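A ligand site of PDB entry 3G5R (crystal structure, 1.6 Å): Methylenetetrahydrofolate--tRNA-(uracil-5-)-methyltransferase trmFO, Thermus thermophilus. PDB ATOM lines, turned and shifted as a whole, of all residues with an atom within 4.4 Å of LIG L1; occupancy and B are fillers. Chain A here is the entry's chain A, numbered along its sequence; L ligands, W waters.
OE2 of Glu 31 sits at hydrogen-bond distance from O5 of LIG L1, at 2.7 Å.
An oxygen (O14) of LIG L1 is in hydrogen-bond range of the backbone NH (N) of Ala 12 (2.8 Å).
The backbone NH (N) of Val 121 sits at hydrogen-bond distance from a nitrogen (N4) of LIG L1 (2.9 Å).
The backbone carbonyl oxygen (O) of Val 121 sits at hydrogen-bond distance from a nitrogen (N3) of LIG L1, 2.9 Å away.
The backbone NH (N) of Val 336 sits at hydrogen-bond distance from an oxygen (O13) of LIG L1 (2.9 Å).
The backbone NH (N) of Ser 138 lies within hydrogen-bond range of a nitrogen (N2) of LIG L1 (3.2 Å).
N3 of LIG L1 lies within hydrogen-bond range of OG of Ser 138 (2.9 Å).
The guanidinium group of Arg 33 sits at hydrogen-bond distance from an oxygen (O5) of LIG L1 (3.0 Å).
An oxygen (O9) of LIG L1 lies close to the backbone NH (N) of Gly 342, 3.1 Å away.
The backbone carbonyl oxygen (O) of Gly 342 sits close to an oxygen (O9) of LIG L1.
The backbone NH of Tyr 343 sits at hydrogen-bond distance from an oxygen (O7) of LIG L1, 3.0 Å away.
O8 of LIG L1 sits close to OH of Tyr 343, at 3.5 Å.
An oxygen (O14) of LIG L1 lies within hydrogen-bond range of the backbone NH of Leu 11, 3.1 Å away.
O8 of LIG L1 sits close to N of Ser 52 (3.2 Å).
N of Met 32 lies within hydrogen-bond range of N5 of LIG L1.
The side-chain hydroxyl (OG) of Ser 346 is in hydrogen-bond range of an oxygen (O12) of LIG L1, at 3.3 Å.
A nitrogen (N8) of LIG L1 sits at hydrogen-bond distance from a nitrogen (N4) of LG2 L2.
O of Glu 31 is in hydrogen-bond range of N of Glu 119 (3.3 Å).
OE2 of Glu 31 lies within hydrogen-bond range of N of Ala 9.
OG of Ser 138 sits at hydrogen-bond distance from OE2 of Glu 120 (2.7 Å).
The backbone carbonyl oxygen (O) of Gly 134 is in hydrogen-bond range of the side-chain hydroxyl (OG1) of Thr 137 (2.8 Å).
The backbone NH of Gly 8 sits at hydrogen-bond distance from the backbone carbonyl oxygen of Phe 30 (2.8 Å).
The backbone carbonyl oxygen (O) of Val 7 lies within hydrogen-bond range of the backbone NH (N) of Ala 132 (2.8 Å).
ND1 of His 41 is in hydrogen-bond range of OG1 of Thr 38 (2.6 Å).
OG1 of Thr 38 sits close to N of Ala 40 (3.1 Å).
An oxygen (O4) of LIG L1 lies close to the backbone carbonyl oxygen (O) of Thr 133 (3.5 Å).
Val 7 touches LIG L1.
Gly 8 touches LIG L1 (CA to O4, 3.3 Å).
Ala 9 touches LIG L1.
CA of Gly 10 touches O3 of LIG L1 (3.2 Å).
Thr 38 touches LIG L1.
CE1 of His 41 touches O1 of LIG L1, 3.4 Å away.
Val 50 touches LIG L1 (CG2 to C15, 3.9 Å).
Cys 51 touches LIG L1.
Glu 119 touches LIG L1.
CA of Glu 120 touches N4 of LIG L1, at 3.7 Å.
O of Ala 132 touches C1 of LIG L1, at 3.4 Å.
Gly 134 touches LIG L1.
Pro 135 touches LIG L1 (CG to O10, 3.4 Å).
CA of Thr 137 touches N2 of LIG L1 (3.8 Å).
CB of Leu 141 touches N3 of LIG L1 (3.9 Å).
Gly 335 touches LIG L1.
Within 4 Å of LIG L1: Val 7, Gly 8, Ala 9, Gly 10, Leu 11, Ala 12, Glu 31, Met 32, Arg 33, Thr 38, His 41, Val 50, Cys 51, Ser 52, Glu 119, Glu 120, Val 121, Ala 132, Thr 133, Gly 134, Pro 135, Thr 137, Ser 138, Leu 141, Gly 335, Val 336, Gly 342, Tyr 343 and Ser 346.
The nearest printed residue that does not touch LIG L1 is Leu 136 (4.1 Å).
Water W5 lies within hydrogen-bond range of O11 of LIG L1 (2.7 Å) and N of Val 50 (3.2 Å).
Water W10 lies within hydrogen-bond range of O13 of LIG L1 (2.7 Å), N of Gly 134 (2.9 Å) and N of Val 336 (3.2 Å).
Water W2 lies within hydrogen-bond range of O2 of LIG L1 (2.7 Å) and NE2 of His 41 (2.9 Å).
Water W7 lies within hydrogen-bond range of a nitrogen (N7) of LIG L1 (2.9 Å) and the side-chain hydroxyl of Ser 52 (3.3 Å).
Water W1 lies within hydrogen-bond range of N of Leu 136 (2.8 Å), O1 of LIG L1 (2.9 Å) and O of Thr 133 (2.9 Å).
Water W3 bridges an oxygen (O1) of LG2 L2 (2.6 Å) and a nitrogen (N7) of LIG L1 (3.4 Å).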
ATOM      1  N   VAL A   7     -26.773 -25.642 -35.301  1.00  0.00           N
ATOM      2  CA  VAL A   7     -26.417 -24.756 -34.197  1.00  0.00           C
ATOM      3  C   VAL A   7     -25.230 -25.303 -33.413  1.00  0.00           C
ATOM      4  O   VAL A   7     -25.338 -26.312 -32.715  1.00  0.00           O
ATOM      5  CB  VAL A   7     -27.600 -24.510 -33.256  1.00  0.00           C
ATOM      6  CG1 VAL A   7     -27.233 -23.481 -32.193  1.00  0.00           C
ATOM      7  CG2 VAL A   7     -28.813 -24.033 -34.054  1.00  0.00           C
ATOM      8  N   GLY A   8     -24.096 -24.617 -33.540  1.00  0.00           N
ATOM      9  CA  GLY A   8     -22.855 -25.040 -32.933  1.00  0.00           C
ATOM     10  C   GLY A   8     -21.930 -25.625 -33.988  1.00  0.00           C
ATOM     11  O   GLY A   8     -22.325 -26.527 -34.725  1.00  0.00           O
ATOM     12  N   ALA A   9     -20.723 -25.087 -34.076  1.00  0.00           N
ATOM     13  CA  ALA A   9     -19.744 -25.532 -35.062  1.00  0.00           C
ATOM     14  C   ALA A   9     -18.566 -26.199 -34.369  1.00  0.00           C
ATOM     15  O   ALA A   9     -17.408 -25.875 -34.641  1.00  0.00           O
ATOM     16  CB  ALA A   9     -19.263 -24.363 -35.919  1.00  0.00           C
ATOM     17  N   GLY A  10     -18.869 -27.121 -33.453  1.00  0.00           N
ATOM     18  CA  GLY A  10     -17.849 -27.929 -32.807  1.00  0.00           C
ATOM     19  C   GLY A  10     -17.641 -29.211 -33.590  1.00  0.00           C
ATOM     20  O   GLY A  10     -17.782 -29.230 -34.808  1.00  0.00           O
ATOM     21  N   LEU A  11     -17.303 -30.290 -32.896  1.00  0.00           N
ATOM     22  CA  LEU A  11     -17.059 -31.563 -33.574  1.00  0.00           C
ATOM     23  C   LEU A  11     -18.316 -32.060 -34.284  1.00  0.00           C
ATOM     24  O   LEU A  11     -18.290 -32.448 -35.445  1.00  0.00           O
ATOM     25  CB  LEU A  11     -16.563 -32.622 -32.589  1.00  0.00           C
ATOM     26  CG  LEU A  11     -15.068 -32.639 -32.242  1.00  0.00           C
ATOM     27  CD1 LEU A  11     -14.255 -33.179 -33.414  1.00  0.00           C
ATOM     28  CD2 LEU A  11     -14.578 -31.261 -31.821  1.00  0.00           C
ATOM     29  N   ALA A  12     -19.437 -32.043 -33.564  1.00  0.00           N
ATOM     30  CA  ALA A  12     -20.682 -32.581 -34.095  1.00  0.00           C
ATOM     31  C   ALA A  12     -21.263 -31.678 -35.188  1.00  0.00           C
ATOM     32  O   ALA A  12     -21.651 -32.167 -36.252  1.00  0.00           O
ATOM     33  CB  ALA A  12     -21.684 -32.767 -32.971  1.00  0.00           C
ATOM     34  N   GLY A  13     -21.315 -30.378 -34.908  1.00  0.00           N
ATOM     35  CA  GLY A  13     -21.896 -29.427 -35.849  1.00  0.00           C
ATOM     36  C   GLY A  13     -21.136 -29.332 -37.156  1.00  0.00           C
ATOM     37  O   GLY A  13     -21.740 -29.227 -38.231  1.00  0.00           O
ATOM     38  N   PHE A  30     -24.613 -21.754 -37.279  1.00  0.00           N
ATOM     39  CA  PHE A  30     -24.463 -20.771 -36.211  1.00  0.00           C
ATOM     40  C   PHE A  30     -23.307 -21.174 -35.314  1.00  0.00           C
ATOM     41  O   PHE A  30     -23.204 -22.330 -34.911  1.00  0.00           O
ATOM     42  CB  PHE A  30     -25.729 -20.687 -35.356  1.00  0.00           C
ATOM     43  CG  PHE A  30     -26.928 -20.144 -36.088  1.00  0.00           C
ATOM     44  CD1 PHE A  30     -27.749 -21.002 -36.802  1.00  0.00           C
ATOM     45  CD2 PHE A  30     -27.236 -18.806 -36.040  1.00  0.00           C
ATOM     46  CE1 PHE A  30     -28.864 -20.516 -37.469  1.00  0.00           C
ATOM     47  CE2 PHE A  30     -28.348 -18.308 -36.699  1.00  0.00           C
ATOM     48  CZ  PHE A  30     -29.160 -19.169 -37.412  1.00  0.00           C
ATOM     49  N   GLU A  31     -22.436 -20.215 -35.010  1.00  0.00           N
ATOM     50  CA  GLU A  31     -21.374 -20.430 -34.029  1.00  0.00           C
ATOM     51  C   GLU A  31     -21.196 -19.143 -33.234  1.00  0.00           C
ATOM     52  O   GLU A  31     -20.880 -18.099 -33.809  1.00  0.00           O
ATOM     53  CB  GLU A  31     -20.070 -20.816 -34.711  1.00  0.00           C
ATOM     54  CG  GLU A  31     -18.888 -20.909 -33.744  1.00  0.00           C
ATOM     55  CD  GLU A  31     -19.200 -21.752 -32.527  1.00  0.00           C
ATOM     56  OE1 GLU A  31     -19.124 -21.238 -31.394  1.00  0.00           O
ATOM     57  OE2 GLU A  31     -19.536 -22.948 -32.695  1.00  0.00           O
ATOM     58  N   MET A  32     -21.379 -19.222 -31.923  1.00  0.00           N
ATOM     59  CA  MET A  32     -21.306 -18.015 -31.103  1.00  0.00           C
ATOM     60  C   MET A  32     -19.873 -17.494 -30.927  1.00  0.00           C
ATOM     61  O   MET A  32     -19.674 -16.298 -30.741  1.00  0.00           O
ATOM     62  CB  MET A  32     -21.986 -18.217 -29.759  1.00  0.00           C
ATOM     63  CG  MET A  32     -21.247 -19.164 -28.826  1.00  0.00           C
ATOM     64  SD  MET A  32     -22.181 -19.385 -27.301  1.00  0.00           S
ATOM     65  CE  MET A  32     -21.036 -20.379 -26.350  1.00  0.00           C
ATOM     66  N   ARG A  33     -18.896 -18.389 -30.991  1.00  0.00           N
ATOM     67  CA  ARG A  33     -17.491 -17.958 -30.916  1.00  0.00           C
ATOM     68  C   ARG A  33     -17.101 -17.183 -32.169  1.00  0.00           C
ATOM     69  O   ARG A  33     -17.479 -17.562 -33.274  1.00  0.00           O
ATOM     70  CB  ARG A  33     -16.561 -19.168 -30.737  1.00  0.00           C
ATOM     71  CG  ARG A  33     -16.827 -19.950 -29.461  1.00  0.00           C
ATOM     72  CD  ARG A  33     -15.896 -21.143 -29.307  1.00  0.00           C
ATOM     73  NE  ARG A  33     -16.206 -22.232 -30.234  1.00  0.00           N
ATOM     74  CZ  ARG A  33     -15.409 -22.640 -31.226  1.00  0.00           C
ATOM     75  NH1 ARG A  33     -14.246 -22.034 -31.442  1.00  0.00           N
ATOM     76  NH2 ARG A  33     -15.781 -23.642 -32.005  1.00  0.00           N
ATOM     77  N   THR A  38     -17.081 -20.107 -24.656  1.00  0.00           N
ATOM     78  CA  THR A  38     -17.316 -21.039 -23.564  1.00  0.00           C
ATOM     79  C   THR A  38     -16.099 -20.991 -22.645  1.00  0.00           C
ATOM     80  O   THR A  38     -15.055 -20.459 -23.018  1.00  0.00           O
ATOM     81  CB  THR A  38     -17.431 -22.489 -24.077  1.00  0.00           C
ATOM     82  OG1 THR A  38     -16.119 -22.972 -24.407  1.00  0.00           O
ATOM     83  CG2 THR A  38     -18.346 -22.566 -25.285  1.00  0.00           C
ATOM     84  N   ALA A  40     -14.168 -23.358 -21.992  1.00  0.00           N
ATOM     85  CA  ALA A  40     -13.147 -24.310 -22.433  1.00  0.00           C
ATOM     86  C   ALA A  40     -12.448 -23.899 -23.720  1.00  0.00           C
ATOM     87  O   ALA A  40     -11.322 -24.312 -23.972  1.00  0.00           O
ATOM     88  CB  ALA A  40     -13.754 -25.704 -22.588  1.00  0.00           C
ATOM     89  N   HIS A  41     -13.128 -23.100 -24.543  1.00  0.00           N
ATOM     90  CA  HIS A  41     -12.603 -22.749 -25.849  1.00  0.00           C
ATOM     91  C   HIS A  41     -11.677 -21.540 -25.801  1.00  0.00           C
ATOM     92  O   HIS A  41     -11.833 -20.660 -24.950  1.00  0.00           O
ATOM     93  CB  HIS A  41     -13.761 -22.464 -26.817  1.00  0.00           C
ATOM     94  CG  HIS A  41     -14.472 -23.688 -27.302  1.00  0.00           C
ATOM     95  ND1 HIS A  41     -15.436 -24.326 -26.568  1.00  0.00           N
ATOM     96  CD2 HIS A  41     -14.368 -24.374 -28.474  1.00  0.00           C
ATOM     97  CE1 HIS A  41     -15.907 -25.361 -27.252  1.00  0.00           C
ATOM     98  NE2 HIS A  41     -15.269 -25.411 -28.414  1.00  0.00           N
ATOM     99  N   VAL A  50     -10.619 -29.008 -27.386  1.00  0.00           N
ATOM    100  CA  VAL A  50     -10.387 -28.208 -26.175  1.00  0.00           C
ATOM    101  C   VAL A  50      -9.446 -28.828 -25.140  1.00  0.00           C
ATOM    102  O   VAL A  50      -8.983 -28.133 -24.244  1.00  0.00           O
ATOM    103  CB  VAL A  50     -11.710 -27.809 -25.477  1.00  0.00           C
ATOM    104  CG1 VAL A  50     -12.545 -26.926 -26.390  1.00  0.00           C
ATOM    105  CG2 VAL A  50     -12.482 -29.035 -25.027  1.00  0.00           C
ATOM    106  N   CYS A  51      -9.163 -30.126 -25.254  1.00  0.00           N
ATOM    107  CA  CYS A  51      -8.316 -30.783 -24.270  1.00  0.00           C
ATOM    108  C   CYS A  51      -7.312 -31.742 -24.908  1.00  0.00           C
ATOM    109  O   CYS A  51      -6.424 -31.316 -25.641  1.00  0.00           O
ATOM    110  CB  CYS A  51      -9.167 -31.498 -23.222  1.00  0.00           C
ATOM    111  SG  CYS A  51      -8.297 -31.868 -21.671  1.00  0.00           S
ATOM    112  N   SER A  52      -7.440 -33.034 -24.622  1.00  0.00           N
ATOM    113  CA  SER A  52      -6.545 -34.039 -25.194  1.00  0.00           C
ATOM    114  C   SER A  52      -6.578 -34.004 -26.721  1.00  0.00           C
ATOM    115  O   SER A  52      -7.615 -33.717 -27.313  1.00  0.00           O
ATOM    116  CB  SER A  52      -6.914 -35.442 -24.709  1.00  0.00           C
ATOM    117  OG  SER A  52      -6.194 -36.436 -25.425  1.00  0.00           O
ATOM    118  N   GLU A 119     -23.250 -15.797 -34.220  1.00  0.00           N
ATOM    119  CA  GLU A 119     -24.120 -15.276 -33.184  1.00  0.00           C
ATOM    120  C   GLU A 119     -24.502 -16.381 -32.201  1.00  0.00           C
ATOM    121  O   GLU A 119     -24.475 -17.563 -32.549  1.00  0.00           O
ATOM    122  CB  GLU A 119     -25.402 -14.710 -33.794  1.00  0.00           C
ATOM    123  CG  GLU A 119     -25.183 -13.575 -34.779  1.00  0.00           C
ATOM    124  CD  GLU A 119     -24.838 -12.259 -34.102  1.00  0.00           C
ATOM    125  OE1 GLU A 119     -24.398 -11.325 -34.801  1.00  0.00           O
ATOM    126  OE2 GLU A 119     -25.012 -12.167 -32.860  1.00  0.00           O
ATOM    127  N   GLU A 120     -24.847 -15.989 -30.976  1.00  0.00           N
ATOM    128  CA  GLU A 120     -25.442 -16.941 -30.046  1.00  0.00           C
ATOM    129  C   GLU A 120     -26.909 -17.171 -30.382  1.00  0.00           C
ATOM    130  O   GLU A 120     -27.689 -16.223 -30.473  1.00  0.00           O
ATOM    131  CB  GLU A 120     -25.318 -16.475 -28.603  1.00  0.00           C
ATOM    132  CG  GLU A 120     -25.918 -17.468 -27.619  1.00  0.00           C
ATOM    133  CD  GLU A 120     -26.130 -16.882 -26.230  1.00  0.00           C
ATOM    134  OE1 GLU A 120     -25.873 -15.679 -26.040  1.00  0.00           O
ATOM    135  OE2 GLU A 120     -26.567 -17.635 -25.342  1.00  0.00           O
ATOM    136  N   VAL A 121     -27.269 -18.439 -30.572  1.00  0.00           N
ATOM    137  CA  VAL A 121     -28.658 -18.820 -30.733  1.00  0.00           C
ATOM    138  C   VAL A 121     -29.314 -18.946 -29.356  1.00  0.00           C
ATOM    139  O   VAL A 121     -28.845 -19.710 -28.510  1.00  0.00           O
ATOM    140  CB  VAL A 121     -28.766 -20.146 -31.511  1.00  0.00           C
ATOM    141  CG1 VAL A 121     -30.189 -20.681 -31.494  1.00  0.00           C
ATOM    142  CG2 VAL A 121     -28.255 -19.962 -32.927  1.00  0.00           C
ATOM    143  N   ALA A 132     -26.312 -28.809 -31.846  1.00  0.00           N
ATOM    144  CA  ALA A 132     -25.015 -29.433 -31.583  1.00  0.00           C
ATOM    145  C   ALA A 132     -24.158 -28.506 -30.749  1.00  0.00           C
ATOM    146  O   ALA A 132     -23.019 -28.214 -31.097  1.00  0.00           O
ATOM    147  CB  ALA A 132     -24.321 -29.771 -32.896  1.00  0.00           C
ATOM    148  N   THR A 133     -24.702 -28.038 -29.637  1.00  0.00           N
ATOM    149  CA  THR A 133     -24.082 -26.953 -28.880  1.00  0.00           C
ATOM    150  C   THR A 133     -23.139 -27.422 -27.774  1.00  0.00           C
ATOM    151  O   THR A 133     -22.519 -26.596 -27.110  1.00  0.00           O
ATOM    152  CB  THR A 133     -25.151 -26.008 -28.328  1.00  0.00           C
ATOM    153  OG1 THR A 133     -26.245 -26.775 -27.808  1.00  0.00           O
ATOM    154  CG2 THR A 133     -25.651 -25.102 -29.436  1.00  0.00           C
ATOM    155  N   GLY A 134     -23.026 -28.731 -27.566  1.00  0.00           N
ATOM    156  CA  GLY A 134     -21.943 -29.283 -26.769  1.00  0.00           C
ATOM    157  C   GLY A 134     -22.095 -29.214 -25.257  1.00  0.00           C
ATOM    158  O   GLY A 134     -23.135 -28.813 -24.754  1.00  0.00           O
ATOM    159  N   PRO A 135     -21.040 -29.601 -24.530  1.00  0.00           N
ATOM    160  CA  PRO A 135     -21.112 -29.681 -23.062  1.00  0.00           C
ATOM    161  C   PRO A 135     -21.301 -28.301 -22.441  1.00  0.00           C
ATOM    162  O   PRO A 135     -21.823 -28.183 -21.331  1.00  0.00           O
ATOM    163  CB  PRO A 135     -19.737 -30.245 -22.684  1.00  0.00           C
ATOM    164  CG  PRO A 135     -18.849 -29.846 -23.847  1.00  0.00           C
ATOM    165  CD  PRO A 135     -19.734 -30.078 -25.029  1.00  0.00           C
ATOM    166  N   LEU A 136     -20.888 -27.259 -23.163  1.00  0.00           N
ATOM    167  CA  LEU A 136     -20.996 -25.899 -22.654  1.00  0.00           C
ATOM    168  C   LEU A 136     -21.995 -25.079 -23.489  1.00  0.00           C
ATOM    169  O   LEU A 136     -21.776 -23.903 -23.755  1.00  0.00           O
ATOM    170  CB  LEU A 136     -19.621 -25.238 -22.617  1.00  0.00           C
ATOM    171  CG  LEU A 136     -18.613 -25.982 -21.729  1.00  0.00           C
ATOM    172  CD1 LEU A 136     -17.218 -25.380 -21.851  1.00  0.00           C
ATOM    173  CD2 LEU A 136     -19.092 -25.992 -20.286  1.00  0.00           C
ATOM    174  N   THR A 137     -23.065 -25.748 -23.904  1.00  0.00           N
ATOM    175  CA  THR A 137     -24.231 -25.107 -24.495  1.00  0.00           C
ATOM    176  C   THR A 137     -24.572 -23.834 -23.721  1.00  0.00           C
ATOM    177  O   THR A 137     -24.640 -23.860 -22.487  1.00  0.00           O
ATOM    178  CB  THR A 137     -25.455 -26.054 -24.447  1.00  0.00           C
ATOM    179  OG1 THR A 137     -25.245 -27.152 -25.356  1.00  0.00           O
ATOM    180  CG2 THR A 137     -26.746 -25.314 -24.826  1.00  0.00           C
ATOM    181  N   SER A 138     -24.762 -22.725 -24.432  1.00  0.00           N
ATOM    182  CA  SER A 138     -25.034 -21.443 -23.769  1.00  0.00           C
ATOM    183  C   SER A 138     -26.259 -21.556 -22.854  1.00  0.00           C
ATOM    184  O   SER A 138     -27.171 -22.329 -23.120  1.00  0.00           O
ATOM    185  CB  SER A 138     -25.242 -20.325 -24.798  1.00  0.00           C
ATOM    186  OG  SER A 138     -26.563 -20.335 -25.298  1.00  0.00           O
ATOM    187  N   LEU A 141     -29.802 -21.109 -24.477  1.00  0.00           N
ATOM    188  CA  LEU A 141     -30.366 -22.201 -25.248  1.00  0.00           C
ATOM    189  C   LEU A 141     -30.726 -23.369 -24.339  1.00  0.00           C
ATOM    190  O   LEU A 141     -31.716 -24.074 -24.569  1.00  0.00           O
ATOM    191  CB  LEU A 141     -29.411 -22.653 -26.349  1.00  0.00           C
ATOM    192  CG  LEU A 141     -30.001 -23.688 -27.305  1.00  0.00           C
ATOM    193  CD1 LEU A 141     -31.228 -23.111 -27.997  1.00  0.00           C
ATOM    194  CD2 LEU A 141     -28.962 -24.115 -28.333  1.00  0.00           C
ATOM    195  N   GLY A 335     -23.768 -34.819 -30.908  1.00  0.00           N
ATOM    196  CA  GLY A 335     -22.673 -34.516 -30.010  1.00  0.00           C
ATOM    197  C   GLY A 335     -23.048 -34.698 -28.561  1.00  0.00           C
ATOM    198  O   GLY A 335     -23.983 -35.434 -28.213  1.00  0.00           O
ATOM    199  N   VAL A 336     -22.303 -34.026 -27.685  1.00  0.00           N
ATOM    200  CA  VAL A 336     -22.534 -34.130 -26.245  1.00  0.00           C
ATOM    201  C   VAL A 336     -23.978 -33.790 -25.876  1.00  0.00           C
ATOM    202  O   VAL A 336     -24.566 -34.432 -25.003  1.00  0.00           O
ATOM    203  CB  VAL A 336     -21.557 -33.221 -25.490  1.00  0.00           C
ATOM    204  CG1 VAL A 336     -22.037 -32.977 -24.068  1.00  0.00           C
ATOM    205  CG2 VAL A 336     -20.152 -33.846 -25.488  1.00  0.00           C
ATOM    206  N   GLU A 341     -20.208 -38.886 -25.436  1.00  0.00           N
ATOM    207  CA  GLU A 341     -18.991 -38.316 -24.917  1.00  0.00           C
ATOM    208  C   GLU A 341     -17.856 -38.732 -25.856  1.00  0.00           C
ATOM    209  O   GLU A 341     -17.785 -39.892 -26.268  1.00  0.00           O
ATOM    210  CB  GLU A 341     -18.730 -38.844 -23.500  1.00  0.00           C
ATOM    211  CG  GLU A 341     -17.363 -38.538 -22.902  1.00  0.00           C
ATOM    212  CD  GLU A 341     -17.183 -39.113 -21.510  1.00  0.00           C
ATOM    213  OE1 GLU A 341     -18.139 -39.047 -20.695  1.00  0.00           O
ATOM    214  OE2 GLU A 341     -16.081 -39.625 -21.203  1.00  0.00           O
ATOM    215  N   GLY A 342     -17.004 -37.783 -26.230  1.00  0.00           N
ATOM    216  CA  GLY A 342     -15.845 -38.060 -27.060  1.00  0.00           C
ATOM    217  C   GLY A 342     -15.884 -37.277 -28.353  1.00  0.00           C
ATOM    218  O   GLY A 342     -16.958 -37.105 -28.937  1.00  0.00           O
ATOM    219  N   TYR A 343     -14.721 -36.819 -28.809  1.00  0.00           N
ATOM    220  CA  TYR A 343     -14.651 -36.040 -30.050  1.00  0.00           C
ATOM    221  C   TYR A 343     -15.237 -36.825 -31.224  1.00  0.00           C
ATOM    222  O   TYR A 343     -16.044 -36.317 -32.005  1.00  0.00           O
ATOM    223  CB  TYR A 343     -13.212 -35.681 -30.390  1.00  0.00           C
ATOM    224  CG  TYR A 343     -12.426 -34.927 -29.336  1.00  0.00           C
ATOM    225  CD1 TYR A 343     -12.876 -33.722 -28.813  1.00  0.00           C
ATOM    226  CD2 TYR A 343     -11.187 -35.395 -28.914  1.00  0.00           C
ATOM    227  CE1 TYR A 343     -12.120 -33.016 -27.873  1.00  0.00           C
ATOM    228  CE2 TYR A 343     -10.443 -34.719 -27.977  1.00  0.00           C
ATOM    229  CZ  TYR A 343     -10.908 -33.533 -27.471  1.00  0.00           C
ATOM    230  OH  TYR A 343     -10.132 -32.859 -26.530  1.00  0.00           O
ATOM    231  N   SER A 346     -18.924 -37.523 -31.069  1.00  0.00           N
ATOM    232  CA  SER A 346     -19.635 -36.298 -31.369  1.00  0.00           C
ATOM    233  C   SER A 346     -19.673 -36.054 -32.883  1.00  0.00           C
ATOM    234  O   SER A 346     -20.729 -35.773 -33.444  1.00  0.00           O
ATOM    235  CB  SER A 346     -19.002 -35.113 -30.640  1.00  0.00           C
ATOM    236  OG  SER A 346     -19.117 -35.303 -29.238  1.00  0.00           O
HETATM  237  P1  LIG L   1     -18.343 -28.675 -28.920  1.00  0.00           P
HETATM  238  O1  LIG L   1     -18.089 -27.965 -27.618  1.00  0.00           O
HETATM  239  O2  LIG L   1     -17.111 -29.170 -29.629  1.00  0.00           O
HETATM  240  O3  LIG L   1     -19.132 -27.701 -29.927  1.00  0.00           O
HETATM  241  C1  LIG L   1     -20.278 -27.015 -29.516  1.00  0.00           C
HETATM  242  C2  LIG L   1     -20.217 -25.652 -30.194  1.00  0.00           C
HETATM  243  O4  LIG L   1     -21.438 -24.978 -29.974  1.00  0.00           O
HETATM  244  C3  LIG L   1     -19.115 -24.762 -29.600  1.00  0.00           C
HETATM  245  O5  LIG L   1     -18.346 -24.225 -30.656  1.00  0.00           O
HETATM  246  C4  LIG L   1     -19.869 -23.660 -28.876  1.00  0.00           C
HETATM  247  O6  LIG L   1     -19.199 -22.425 -28.972  1.00  0.00           O
HETATM  248  C5  LIG L   1     -21.167 -23.629 -29.669  1.00  0.00           C
HETATM  249  N1  LIG L   1     -22.351 -23.101 -28.965  1.00  0.00           N
HETATM  250  C6  LIG L   1     -22.777 -23.394 -27.697  1.00  0.00           C
HETATM  251  N2  LIG L   1     -23.931 -22.718 -27.482  1.00  0.00           N
HETATM  252  C7  LIG L   1     -24.251 -22.021 -28.598  1.00  0.00           C
HETATM  253  C8  LIG L   1     -25.296 -21.168 -28.925  1.00  0.00           C
HETATM  254  N3  LIG L   1     -26.360 -21.079 -28.126  1.00  0.00           N
HETATM  255  N4  LIG L   1     -25.341 -20.600 -30.188  1.00  0.00           N
HETATM  256  C9  LIG L   1     -24.331 -20.851 -31.102  1.00  0.00           C
HETATM  257  N5  LIG L   1     -23.291 -21.689 -30.769  1.00  0.00           N
HETATM  258  C10 LIG L   1     -23.262 -22.258 -29.538  1.00  0.00           C
HETATM  259  N6  LIG L   1     -13.557 -35.318 -25.336  1.00  0.00           N
HETATM  260  C11 LIG L   1     -12.568 -36.203 -25.704  1.00  0.00           C
HETATM  261  O7  LIG L   1     -12.809 -37.111 -26.498  1.00  0.00           O
HETATM  262  N7  LIG L   1     -11.302 -36.088 -25.154  1.00  0.00           N
HETATM  263  C12 LIG L   1     -11.034 -35.068 -24.264  1.00  0.00           C
HETATM  264  O8  LIG L   1      -9.907 -34.952 -23.790  1.00  0.00           O
HETATM  265  C13 LIG L   1     -12.037 -34.169 -23.912  1.00  0.00           C
HETATM  266  N8  LIG L   1     -11.769 -33.145 -23.012  1.00  0.00           N
HETATM  267  C14 LIG L   1     -12.773 -32.263 -22.686  1.00  0.00           C
HETATM  268  C15 LIG L   1     -12.506 -31.240 -21.786  1.00  0.00           C
HETATM  269  C16 LIG L   1     -13.504 -30.335 -21.446  1.00  0.00           C
HETATM  270  C17 LIG L   1     -13.206 -29.229 -20.473  1.00  0.00           C
HETATM  271  C18 LIG L   1     -14.777 -30.468 -21.991  1.00  0.00           C
HETATM  272  C19 LIG L   1     -15.866 -29.503 -21.623  1.00  0.00           C
HETATM  273  C20 LIG L   1     -15.044 -31.491 -22.890  1.00  0.00           C
HETATM  274  C21 LIG L   1     -14.046 -32.399 -23.241  1.00  0.00           C
HETATM  275  N9  LIG L   1     -14.332 -33.434 -24.128  1.00  0.00           N
HETATM  276  C22 LIG L   1     -13.306 -34.293 -24.459  1.00  0.00           C
HETATM  277  C23 LIG L   1     -15.744 -33.927 -24.290  1.00  0.00           C
HETATM  278  C24 LIG L   1     -16.313 -33.836 -25.724  1.00  0.00           C
HETATM  279  O9  LIG L   1     -15.922 -34.927 -26.535  1.00  0.00           O
HETATM  280  C25 LIG L   1     -15.921 -32.525 -26.399  1.00  0.00           C
HETATM  281  O10 LIG L   1     -16.498 -31.467 -25.658  1.00  0.00           O
HETATM  282  C26 LIG L   1     -16.379 -32.447 -27.862  1.00  0.00           C
HETATM  283  O11 LIG L   1     -15.818 -31.293 -28.446  1.00  0.00           O
HETATM  284  C27 LIG L   1     -17.896 -32.358 -27.959  1.00  0.00           C
HETATM  285  O12 LIG L   1     -18.286 -32.078 -29.296  1.00  0.00           O
HETATM  286  P2  LIG L   1     -19.596 -31.184 -29.544  1.00  0.00           P
HETATM  287  O13 LIG L   1     -20.778 -31.917 -28.958  1.00  0.00           O
HETATM  288  O14 LIG L   1     -19.708 -30.825 -31.004  1.00  0.00           O
HETATM  289  O15 LIG L   1     -19.353 -29.882 -28.611  1.00  0.00           O
HETATM  290  N1  LG2 L   2     -16.478 -34.088 -20.905  1.00  0.00           N
HETATM  291  C1  LG2 L   2     -16.751 -32.956 -20.210  1.00  0.00           C
HETATM  292  N2  LG2 L   2     -15.765 -32.345 -19.452  1.00  0.00           N
HETATM  293  C2  LG2 L   2     -14.512 -32.870 -19.420  1.00  0.00           C
HETATM  294  C3  LG2 L   2     -14.211 -34.057 -20.149  1.00  0.00           C
HETATM  295  C4  LG2 L   2     -15.170 -34.638 -20.871  1.00  0.00           C
HETATM  296  N3  LG2 L   2     -13.434 -32.218 -18.602  1.00  0.00           N
HETATM  297  C5  LG2 L   2     -12.038 -32.641 -18.848  1.00  0.00           C
HETATM  298  C6  LG2 L   2     -11.973 -34.151 -19.129  1.00  0.00           C
HETATM  299  N4  LG2 L   2     -12.881 -34.584 -20.119  1.00  0.00           N
HETATM  300  O1  LG2 L   2     -14.893 -35.800 -21.589  1.00  0.00           O
HETATM  301  N5  LG2 L   2     -18.077 -32.380 -20.263  1.00  0.00           N
HETATM  302  O   HOH W   1     -19.928 -26.663 -25.775  1.00  0.00           O
HETATM  303  O   HOH W   2     -15.325 -27.321 -30.554  1.00  0.00           O
HETATM  304  O   HOH W   3     -12.630 -36.982 -22.103  1.00  0.00           O
HETATM  305  O   HOH W   4      -8.797 -37.339 -21.868  1.00  0.00           O
HETATM  306  O   HOH W   5     -13.573 -29.811 -28.212  1.00  0.00           O
HETATM  307  O   HOH W   6     -11.383 -39.131 -27.724  1.00  0.00           O
HETATM  308  O   HOH W   7      -9.157 -37.862 -25.958  1.00  0.00           O
HETATM  309  O   HOH W   8     -15.813 -28.896 -26.261  1.00  0.00           O
HETATM  310  O   HOH W   9     -20.814 -28.970 -32.511  1.00  0.00           O
HETATM  311  O   HOH W  10     -23.417 -31.237 -28.897  1.00  0.00           O
